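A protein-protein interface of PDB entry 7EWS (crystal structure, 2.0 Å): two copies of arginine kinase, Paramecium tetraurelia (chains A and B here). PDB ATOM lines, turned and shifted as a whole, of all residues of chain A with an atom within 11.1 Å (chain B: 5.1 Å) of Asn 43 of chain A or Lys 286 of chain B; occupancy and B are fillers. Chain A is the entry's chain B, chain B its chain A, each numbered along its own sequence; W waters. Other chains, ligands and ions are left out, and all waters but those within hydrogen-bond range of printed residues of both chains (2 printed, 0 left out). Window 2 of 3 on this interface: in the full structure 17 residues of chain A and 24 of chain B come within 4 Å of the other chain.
Lys 42 of chain A touches Val 154 of chain B. Lys 42 of chain A touches Lys 286 of chain B (O to CB, 3.7 Å). Asn 43 of chain A touches Val 154 of chain B. Asn 43 of chain A touches Phe 287 of chain B. CA of Ala 288 of chain B touches O of Asn 43 of chain A, at 3.3 Å. CG1 of Val 154 of chain B touches O of Ile 44 of chain A, at 3.8 Å. Ile 44 of chain A touches Glu 289 of chain B (CG1 to O, 3.6 Å).
Water W1 lies within hydrogen-bond range of O of Phe 287 of chain B (2.7 Å) and OD1 of Asn 43 of chain A (2.9 Å). Water W2 lies within hydrogen-bond range of O of Asp 39 of chain A and NZ of Lys 286 of chain B.
No position is printed for both chains. Of the 9 pairs that touch across the chains among the printed residues, none has its exchanged pair printed and touching as well.
Of the printed residues of chain B, Asn 43 of chain A touches Val 154, Lys 286, Phe 287, Ala 288 and Glu 289. Of chain A, only Lys 42 and Asn 43 come within 4 Å of Lys 286 of chain B. No residue of chain A comes within 4 Å of Val 153 of chain B. Of chain A, only Lys 42 (3.4 Å), Asn 43 (3.6 Å) and Ile 44 (3.8 Å) come within 4 Å of Val 154 of chain B. No residue of chain A comes within 4 Å of Leu 285 of chain B. Printed residues of chain A within 4 Å of Phe 287 of chain B: Asn 43. Of the printed residues of chain B, Lys 42 of chain A touches Val 154 (3.4 Å) and Lys 286 (3.7 Å). Of the printed residues of chain A, Glu 289 of chain B touches Asn 43 (2.8 Å) and Ile 44 (3.6 Å). Printed residues of chain B within 4 Å of Ile 44 of chain A: Val 154 and Glu 289. The nearest residue of chain B that does not touch Asn 43 of chain A is Ile 296 of chain B (4.9 Å). The nearest printed residue of chain A that does not touch Glu 289 of chain B is Glu 40 of chain A (5.7 Å).
Of the 10 printed residues of chain B, 5 touch a printed residue of chain A. Printed residues of chain B that touch a printed residue of chain A: Val 154, Lys 286, Phe 287, Ala 288 and Glu 289. Hydrophobic or aromatic side chains of chain B that line the printed part of chain A: Val 154. Of the 16 printed residues of chain A, 3 touch a printed residue of chain B.
O of Asn 152 of chain B is in hydrogen-bond range of N of Ala 288 of chain B (2.9 Å). The backbone NH of Val 154 of chain B lies within hydrogen-bond range of the backbone carbonyl oxygen of Lys 286 of chain B (2.9 Å). The backbone carbonyl oxygen (O) of Ala 288 of chain B is in hydrogen-bond range of the backbone NH (N) of Ile 296 of chain B, at 3.0 Å. The side-chain carboxylate (OD1) of Asp 39 of chain A is in salt-bridge range of the side-chain amino group (NZ) of Lys 42 of chain A. The backbone carbonyl oxygen (O) of Glu 40 of chain A lies within hydrogen-bond range of the side-chain amide nitrogen (ND2) of Asn 43 of chain A (2.9 Å).
NZ of Lys 286 of chain B is in hydrogen-bond range of OD1 of Asn 43 of chain A, 3.1 Å away. The backbone NH of Glu 289 of chain B sits at hydrogen-bond distance from the backbone carbonyl oxygen of Asn 43 of chain A (2.8 Å).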
ATOM      1  N   GLN A  35       3.200  25.430  -8.696  1.00  0.00           N
ATOM      2  CA  GLN A  35       1.800  25.858  -8.950  1.00  0.00           C
ATOM      3  C   GLN A  35       0.924  24.658  -9.340  1.00  0.00           C
ATOM      4  O   GLN A  35      -0.194  24.556  -8.820  1.00  0.00           O
ATOM      5  CB  GLN A  35       1.745  26.947 -10.023  1.00  0.00           C
ATOM      6  CG  GLN A  35       0.344  27.511 -10.202  1.00  0.00           C
ATOM      7  CD  GLN A  35      -0.146  28.137  -8.917  1.00  0.00           C
ATOM      8  OE1 GLN A  35       0.438  29.091  -8.406  1.00  0.00           O
ATOM      9  NE2 GLN A  35      -1.216  27.596  -8.359  1.00  0.00           N
ATOM     10  N   ALA A  36       1.433  23.774 -10.203  1.00  0.00           N
ATOM     11  CA  ALA A  36       0.751  22.537 -10.641  1.00  0.00           C
ATOM     12  C   ALA A  36       0.393  21.691  -9.410  1.00  0.00           C
ATOM     13  O   ALA A  36      -0.734  21.157  -9.351  1.00  0.00           O
ATOM     14  CB  ALA A  36       1.596  21.796 -11.650  1.00  0.00           C
ATOM     15  N   ARG A  37       1.290  21.614  -8.433  1.00  0.00           N
ATOM     16  CA  ARG A  37       1.047  20.845  -7.203  1.00  0.00           C
ATOM     17  C   ARG A  37      -0.038  21.524  -6.349  1.00  0.00           C
ATOM     18  O   ARG A  37      -0.972  20.820  -5.879  1.00  0.00           O
ATOM     19  CB  ARG A  37       2.356  20.668  -6.444  1.00  0.00           C
ATOM     20  CG  ARG A  37       2.170  19.876  -5.164  1.00  0.00           C
ATOM     21  CD  ARG A  37       1.559  18.496  -5.382  1.00  0.00           C
ATOM     22  NE  ARG A  37       1.492  17.851  -4.080  1.00  0.00           N
ATOM     23  CZ  ARG A  37       0.697  16.828  -3.761  1.00  0.00           C
ATOM     24  NH1 ARG A  37      -0.112  16.273  -4.653  1.00  0.00           N
ATOM     25  NH2 ARG A  37       0.707  16.357  -2.533  1.00  0.00           N
ATOM     26  N   TRP A  38       0.059  22.834  -6.132  1.00  0.00           N
ATOM     27  CA  TRP A  38      -1.006  23.578  -5.402  1.00  0.00           C
ATOM     28  C   TRP A  38      -2.369  23.363  -6.096  1.00  0.00           C
ATOM     29  O   TRP A  38      -3.383  23.186  -5.387  1.00  0.00           O
ATOM     30  CB  TRP A  38      -0.708  25.075  -5.327  1.00  0.00           C
ATOM     31  CG  TRP A  38       0.415  25.524  -4.444  1.00  0.00           C
ATOM     32  CD1 TRP A  38       1.263  26.541  -4.771  1.00  0.00           C
ATOM     33  CD2 TRP A  38       0.791  25.093  -3.120  1.00  0.00           C
ATOM     34  NE1 TRP A  38       2.145  26.764  -3.756  1.00  0.00           N
ATOM     35  CE2 TRP A  38       1.893  25.891  -2.734  1.00  0.00           C
ATOM     36  CE3 TRP A  38       0.375  24.087  -2.242  1.00  0.00           C
ATOM     37  CZ2 TRP A  38       2.544  25.745  -1.510  1.00  0.00           C
ATOM     38  CZ3 TRP A  38       1.020  23.935  -1.031  1.00  0.00           C
ATOM     39  CH2 TRP A  38       2.109  24.747  -0.676  1.00  0.00           C
ATOM     40  N   ASP A  39      -2.398  23.398  -7.433  1.00  0.00           N
ATOM     41  CA  ASP A  39      -3.653  23.195  -8.211  1.00  0.00           C
ATOM     42  C   ASP A  39      -4.222  21.792  -7.975  1.00  0.00           C
ATOM     43  O   ASP A  39      -5.442  21.698  -7.858  1.00  0.00           O
ATOM     44  CB  ASP A  39      -3.453  23.476  -9.705  1.00  0.00           C
ATOM     45  CG  ASP A  39      -3.197  24.950  -9.982  1.00  0.00           C
ATOM     46  OD1 ASP A  39      -3.464  25.754  -9.090  1.00  0.00           O
ATOM     47  OD2 ASP A  39      -2.641  25.266 -11.038  1.00  0.00           O
ATOM     48  N   GLU A  40      -3.398  20.738  -7.932  1.00  0.00           N
ATOM     49  CA  GLU A  40      -3.867  19.364  -7.589  1.00  0.00           C
ATOM     50  C   GLU A  40      -4.498  19.366  -6.186  1.00  0.00           C
ATOM     51  O   GLU A  40      -5.548  18.713  -5.976  1.00  0.00           O
ATOM     52  CB  GLU A  40      -2.733  18.334  -7.506  1.00  0.00           C
ATOM     53  CG  GLU A  40      -1.949  18.098  -8.787  1.00  0.00           C
ATOM     54  CD  GLU A  40      -0.624  17.349  -8.608  1.00  0.00           C
ATOM     55  OE1 GLU A  40      -0.462  16.589  -7.570  1.00  0.00           O
ATOM     56  OE2 GLU A  40       0.277  17.542  -9.490  1.00  0.00           O
ATOM     57  N   LEU A  41      -3.819  20.015  -5.240  1.00  0.00           N
ATOM     58  CA  LEU A  41      -4.222  20.005  -3.812  1.00  0.00           C
ATOM     59  C   LEU A  41      -5.574  20.699  -3.654  1.00  0.00           C
ATOM     60  O   LEU A  41      -6.241  20.401  -2.701  1.00  0.00           O
ATOM     61  CB  LEU A  41      -3.126  20.641  -2.945  1.00  0.00           C
ATOM     62  CG  LEU A  41      -1.913  19.730  -2.785  1.00  0.00           C
ATOM     63  CD1 LEU A  41      -0.766  20.411  -2.067  1.00  0.00           C
ATOM     64  CD2 LEU A  41      -2.275  18.425  -2.105  1.00  0.00           C
ATOM     65  N   LYS A  42      -5.974  21.552  -4.597  1.00  0.00           N
ATOM     66  CA  LYS A  42      -7.253  22.298  -4.480  1.00  0.00           C
ATOM     67  C   LYS A  42      -8.414  21.317  -4.579  1.00  0.00           C
ATOM     68  O   LYS A  42      -9.514  21.732  -4.244  1.00  0.00           O
ATOM     69  CB  LYS A  42      -7.390  23.387  -5.541  1.00  0.00           C
ATOM     70  CG  LYS A  42      -6.495  24.582  -5.282  1.00  0.00           C
ATOM     71  CD  LYS A  42      -6.474  25.516  -6.411  1.00  0.00           C
ATOM     72  CE  LYS A  42      -5.442  26.583  -6.144  1.00  0.00           C
ATOM     73  NZ  LYS A  42      -5.332  27.486  -7.305  1.00  0.00           N
ATOM     74  N   ASN A  43      -8.150  20.073  -4.993  1.00  0.00           N
ATOM     75  CA  ASN A  43      -9.178  18.997  -5.055  1.00  0.00           C
ATOM     76  C   ASN A  43      -9.358  18.340  -3.688  1.00  0.00           C
ATOM     77  O   ASN A  43     -10.260  17.514  -3.569  1.00  0.00           O
ATOM     78  CB  ASN A  43      -8.827  17.949  -6.109  1.00  0.00           C
ATOM     79  CG  ASN A  43      -8.734  18.558  -7.487  1.00  0.00           C
ATOM     80  OD1 ASN A  43      -9.733  19.029  -8.009  1.00  0.00           O
ATOM     81  ND2 ASN A  43      -7.541  18.598  -8.058  1.00  0.00           N
ATOM     82  N   ILE A  44      -8.533  18.666  -2.692  1.00  0.00           N
ATOM     83  CA  ILE A  44      -8.592  17.964  -1.377  1.00  0.00           C
ATOM     84  C   ILE A  44      -8.608  18.965  -0.221  1.00  0.00           C
ATOM     85  O   ILE A  44      -9.535  18.902   0.583  1.00  0.00           O
ATOM     86  CB  ILE A  44      -7.460  16.929  -1.250  1.00  0.00           C
ATOM     87  CG1 ILE A  44      -7.700  15.805  -2.261  1.00  0.00           C
ATOM     88  CG2 ILE A  44      -7.337  16.383   0.164  1.00  0.00           C
ATOM     89  CD1 ILE A  44      -6.543  14.877  -2.471  1.00  0.00           C
ATOM     90  N   LYS A  45      -7.576  19.800  -0.114  1.00  0.00           N
ATOM     91  CA  LYS A  45      -7.447  20.781   0.991  1.00  0.00           C
ATOM     92  C   LYS A  45      -6.507  21.903   0.558  1.00  0.00           C
ATOM     93  O   LYS A  45      -5.461  21.598  -0.043  1.00  0.00           O
ATOM     94  CB  LYS A  45      -6.921  20.106   2.256  1.00  0.00           C
ATOM     95  CG  LYS A  45      -6.770  21.012   3.463  1.00  0.00           C
ATOM     96  CD  LYS A  45      -6.185  20.290   4.637  1.00  0.00           C
ATOM     97  CE  LYS A  45      -6.318  21.022   5.952  1.00  0.00           C
ATOM     98  NZ  LYS A  45      -6.331  20.059   7.077  1.00  0.00           N
ATOM     99  N   VAL A  46      -6.894  23.141   0.865  1.00  0.00           N
ATOM    100  CA  VAL A  46      -6.092  24.348   0.550  1.00  0.00           C
ATOM    101  C   VAL A  46      -5.448  24.805   1.861  1.00  0.00           C
ATOM    102  O   VAL A  46      -6.161  25.382   2.711  1.00  0.00           O
ATOM    103  CB  VAL A  46      -6.926  25.487  -0.065  1.00  0.00           C
ATOM    104  CG1 VAL A  46      -6.041  26.699  -0.318  1.00  0.00           C
ATOM    105  CG2 VAL A  46      -7.631  25.069  -1.350  1.00  0.00           C
ATOM    106  N   SER A  47      -4.152  24.554   2.009  1.00  0.00           N
ATOM    107  CA  SER A  47      -3.337  25.064   3.138  1.00  0.00           C
ATOM    108  C   SER A  47      -3.203  26.596   3.027  1.00  0.00           C
ATOM    109  O   SER A  47      -3.409  27.157   1.923  1.00  0.00           O
ATOM    110  CB  SER A  47      -1.990  24.415   3.181  1.00  0.00           C
ATOM    111  OG  SER A  47      -1.257  24.715   1.997  1.00  0.00           O
ATOM    112  N   ASN A  50      -0.741  27.453   0.336  1.00  0.00           N
ATOM    113  CA  ASN A  50      -1.367  27.404  -1.003  1.00  0.00           C
ATOM    114  C   ASN A  50      -2.156  28.709  -1.207  1.00  0.00           C
ATOM    115  O   ASN A  50      -1.953  29.371  -2.213  1.00  0.00           O
ATOM    116  CB  ASN A  50      -2.229  26.139  -1.108  1.00  0.00           C
ATOM    117  CG  ASN A  50      -2.795  25.855  -2.483  1.00  0.00           C
ATOM    118  OD1 ASN A  50      -2.884  26.738  -3.318  1.00  0.00           O
ATOM    119  ND2 ASN A  50      -3.166  24.608  -2.713  1.00  0.00           N
ATOM    120  N   ASP A  83      -1.009  16.625   2.143  1.00  0.00           N
ATOM    121  CA  ASP A  83      -2.268  17.311   1.783  1.00  0.00           C
ATOM    122  C   ASP A  83      -3.170  17.453   3.011  1.00  0.00           C
ATOM    123  O   ASP A  83      -4.219  18.019   2.847  1.00  0.00           O
ATOM    124  CB  ASP A  83      -2.960  16.635   0.606  1.00  0.00           C
ATOM    125  CG  ASP A  83      -3.480  15.242   0.832  1.00  0.00           C
ATOM    126  OD1 ASP A  83      -3.352  14.724   1.974  1.00  0.00           O
ATOM    127  OD2 ASP A  83      -4.016  14.686  -0.182  1.00  0.00           O
ATOM    128  N   ASP A  84      -2.786  16.967   4.189  1.00  0.00           N
ATOM    129  CA  ASP A  84      -3.538  17.277   5.434  1.00  0.00           C
ATOM    130  C   ASP A  84      -3.030  18.594   6.036  1.00  0.00           C
ATOM    131  O   ASP A  84      -3.629  18.998   7.062  1.00  0.00           O
ATOM    132  CB  ASP A  84      -3.517  16.131   6.436  1.00  0.00           C
ATOM    133  CG  ASP A  84      -2.149  15.900   7.075  1.00  0.00           C
ATOM    134  OD1 ASP A  84      -1.149  16.413   6.517  1.00  0.00           O
ATOM    135  OD2 ASP A  84      -2.096  15.237   8.121  1.00  0.00           O
ATOM    136  N   ASN B 152     -18.967  16.348  -1.803  1.00  0.00           N
ATOM    137  CA  ASN B 152     -18.450  17.101  -0.632  1.00  0.00           C
ATOM    138  C   ASN B 152     -17.563  18.237  -1.169  1.00  0.00           C
ATOM    139  O   ASN B 152     -17.076  18.143  -2.334  1.00  0.00           O
ATOM    140  CB  ASN B 152     -17.799  16.186   0.408  1.00  0.00           C
ATOM    141  CG  ASN B 152     -18.803  15.226   1.008  1.00  0.00           C
ATOM    142  OD1 ASN B 152     -19.610  15.619   1.839  1.00  0.00           O
ATOM    143  ND2 ASN B 152     -18.789  13.978   0.566  1.00  0.00           N
ATOM    144  N   VAL B 153     -17.426  19.281  -0.363  1.00  0.00           N
ATOM    145  CA  VAL B 153     -16.844  20.584  -0.750  1.00  0.00           C
ATOM    146  C   VAL B 153     -15.517  20.778  -0.004  1.00  0.00           C
ATOM    147  O   VAL B 153     -15.482  20.635   1.208  1.00  0.00           O
ATOM    148  CB  VAL B 153     -17.851  21.713  -0.481  1.00  0.00           C
ATOM    149  CG1 VAL B 153     -17.252  23.079  -0.783  1.00  0.00           C
ATOM    150  CG2 VAL B 153     -19.130  21.474  -1.264  1.00  0.00           C
ATOM    151  N   VAL B 154     -14.470  21.084  -0.755  1.00  0.00           N
ATOM    152  CA  VAL B 154     -13.113  21.400  -0.229  1.00  0.00           C
ATOM    153  C   VAL B 154     -13.260  22.615   0.705  1.00  0.00           C
ATOM    154  O   VAL B 154     -13.955  23.583   0.314  1.00  0.00           O
ATOM    155  CB  VAL B 154     -12.119  21.645  -1.379  1.00  0.00           C
ATOM    156  CG1 VAL B 154     -10.782  22.172  -0.894  1.00  0.00           C
ATOM    157  CG2 VAL B 154     -11.905  20.394  -2.212  1.00  0.00           C
ATOM    158  N   GLY B 284     -17.402  28.711  -8.007  1.00  0.00           N
ATOM    159  CA  GLY B 284     -15.949  28.660  -7.717  1.00  0.00           C
ATOM    160  C   GLY B 284     -15.574  27.733  -6.555  1.00  0.00           C
ATOM    161  O   GLY B 284     -14.351  27.642  -6.245  1.00  0.00           O
ATOM    162  N   LEU B 285     -16.539  27.092  -5.878  1.00  0.00           N
ATOM    163  CA  LEU B 285     -16.204  26.047  -4.868  1.00  0.00           C
ATOM    164  C   LEU B 285     -15.662  24.830  -5.613  1.00  0.00           C
ATOM    165  O   LEU B 285     -15.888  24.704  -6.845  1.00  0.00           O
ATOM    166  CB  LEU B 285     -17.398  25.683  -3.989  1.00  0.00           C
ATOM    167  CG  LEU B 285     -18.582  24.985  -4.652  1.00  0.00           C
ATOM    168  CD1 LEU B 285     -18.258  23.562  -5.072  1.00  0.00           C
ATOM    169  CD2 LEU B 285     -19.771  24.975  -3.686  1.00  0.00           C
ATOM    170  N   LYS B 286     -14.941  23.980  -4.902  1.00  0.00           N
ATOM    171  CA  LYS B 286     -14.373  22.761  -5.504  1.00  0.00           C
ATOM    172  C   LYS B 286     -14.929  21.567  -4.749  1.00  0.00           C
ATOM    173  O   LYS B 286     -14.969  21.633  -3.523  1.00  0.00           O
ATOM    174  CB  LYS B 286     -12.848  22.704  -5.408  1.00  0.00           C
ATOM    175  CG  LYS B 286     -12.117  23.641  -6.347  1.00  0.00           C
ATOM    176  CD  LYS B 286     -12.040  23.118  -7.746  1.00  0.00           C
ATOM    177  CE  LYS B 286     -11.016  22.022  -7.921  1.00  0.00           C
ATOM    178  NZ  LYS B 286     -10.967  21.565  -9.328  1.00  0.00           N
ATOM    179  N   PHE B 287     -15.185  20.490  -5.484  1.00  0.00           N
ATOM    180  CA  PHE B 287     -15.585  19.195  -4.911  1.00  0.00           C
ATOM    181  C   PHE B 287     -14.320  18.428  -4.529  1.00  0.00           C
ATOM    182  O   PHE B 287     -13.290  18.495  -5.220  1.00  0.00           O
ATOM    183  CB  PHE B 287     -16.531  18.439  -5.847  1.00  0.00           C
ATOM    184  CG  PHE B 287     -17.826  19.150  -6.171  1.00  0.00           C
ATOM    185  CD1 PHE B 287     -18.635  19.704  -5.178  1.00  0.00           C
ATOM    186  CD2 PHE B 287     -18.235  19.273  -7.479  1.00  0.00           C
ATOM    187  CE1 PHE B 287     -19.843  20.318  -5.496  1.00  0.00           C
ATOM    188  CE2 PHE B 287     -19.437  19.894  -7.790  1.00  0.00           C
ATOM    189  CZ  PHE B 287     -20.238  20.418  -6.808  1.00  0.00           C
ATOM    190  N   ALA B 288     -14.427  17.715  -3.415  1.00  0.00           N
ATOM    191  CA  ALA B 288     -13.375  16.843  -2.873  1.00  0.00           C
ATOM    192  C   ALA B 288     -13.242  15.654  -3.827  1.00  0.00           C
ATOM    193  O   ALA B 288     -14.244  14.913  -4.016  1.00  0.00           O
ATOM    194  CB  ALA B 288     -13.719  16.403  -1.483  1.00  0.00           C
ATOM    195  N   GLU B 289     -12.043  15.464  -4.385  1.00  0.00           N
ATOM    196  CA  GLU B 289     -11.779  14.352  -5.315  1.00  0.00           C
ATOM    197  C   GLU B 289     -10.361  13.832  -5.116  1.00  0.00           C
ATOM    198  O   GLU B 289      -9.398  14.650  -5.164  1.00  0.00           O
ATOM    199  CB  GLU B 289     -12.008  14.755  -6.770  1.00  0.00           C
ATOM    200  CG  GLU B 289     -11.840  13.542  -7.647  1.00  0.00           C
ATOM    201  CD  GLU B 289     -12.579  13.506  -8.963  1.00  0.00           C
ATOM    202  OE1 GLU B 289     -12.546  12.410  -9.555  1.00  0.00           O
ATOM    203  OE2 GLU B 289     -13.169  14.553  -9.376  1.00  0.00           O
ATOM    204  N   ILE B 296     -14.798  12.051  -3.421  1.00  0.00           N
ATOM    205  CA  ILE B 296     -14.688  11.743  -1.970  1.00  0.00           C
ATOM    206  C   ILE B 296     -16.069  11.821  -1.313  1.00  0.00           C
ATOM    207  O   ILE B 296     -16.695  12.902  -1.364  1.00  0.00           O
ATOM    208  CB  ILE B 296     -13.627  12.633  -1.291  1.00  0.00           C
ATOM    209  CG1 ILE B 296     -12.225  12.190  -1.748  1.00  0.00           C
ATOM    210  CG2 ILE B 296     -13.795  12.594   0.231  1.00  0.00           C
ATOM    211  CD1 ILE B 296     -11.106  13.158  -1.404  1.00  0.00           C
HETATM  212  O   HOH W   1     -12.590  18.860  -7.784  1.00  0.00           O
HETATM  213  O   HOH W   2      -7.763  22.609  -9.195  1.00  0.00           O
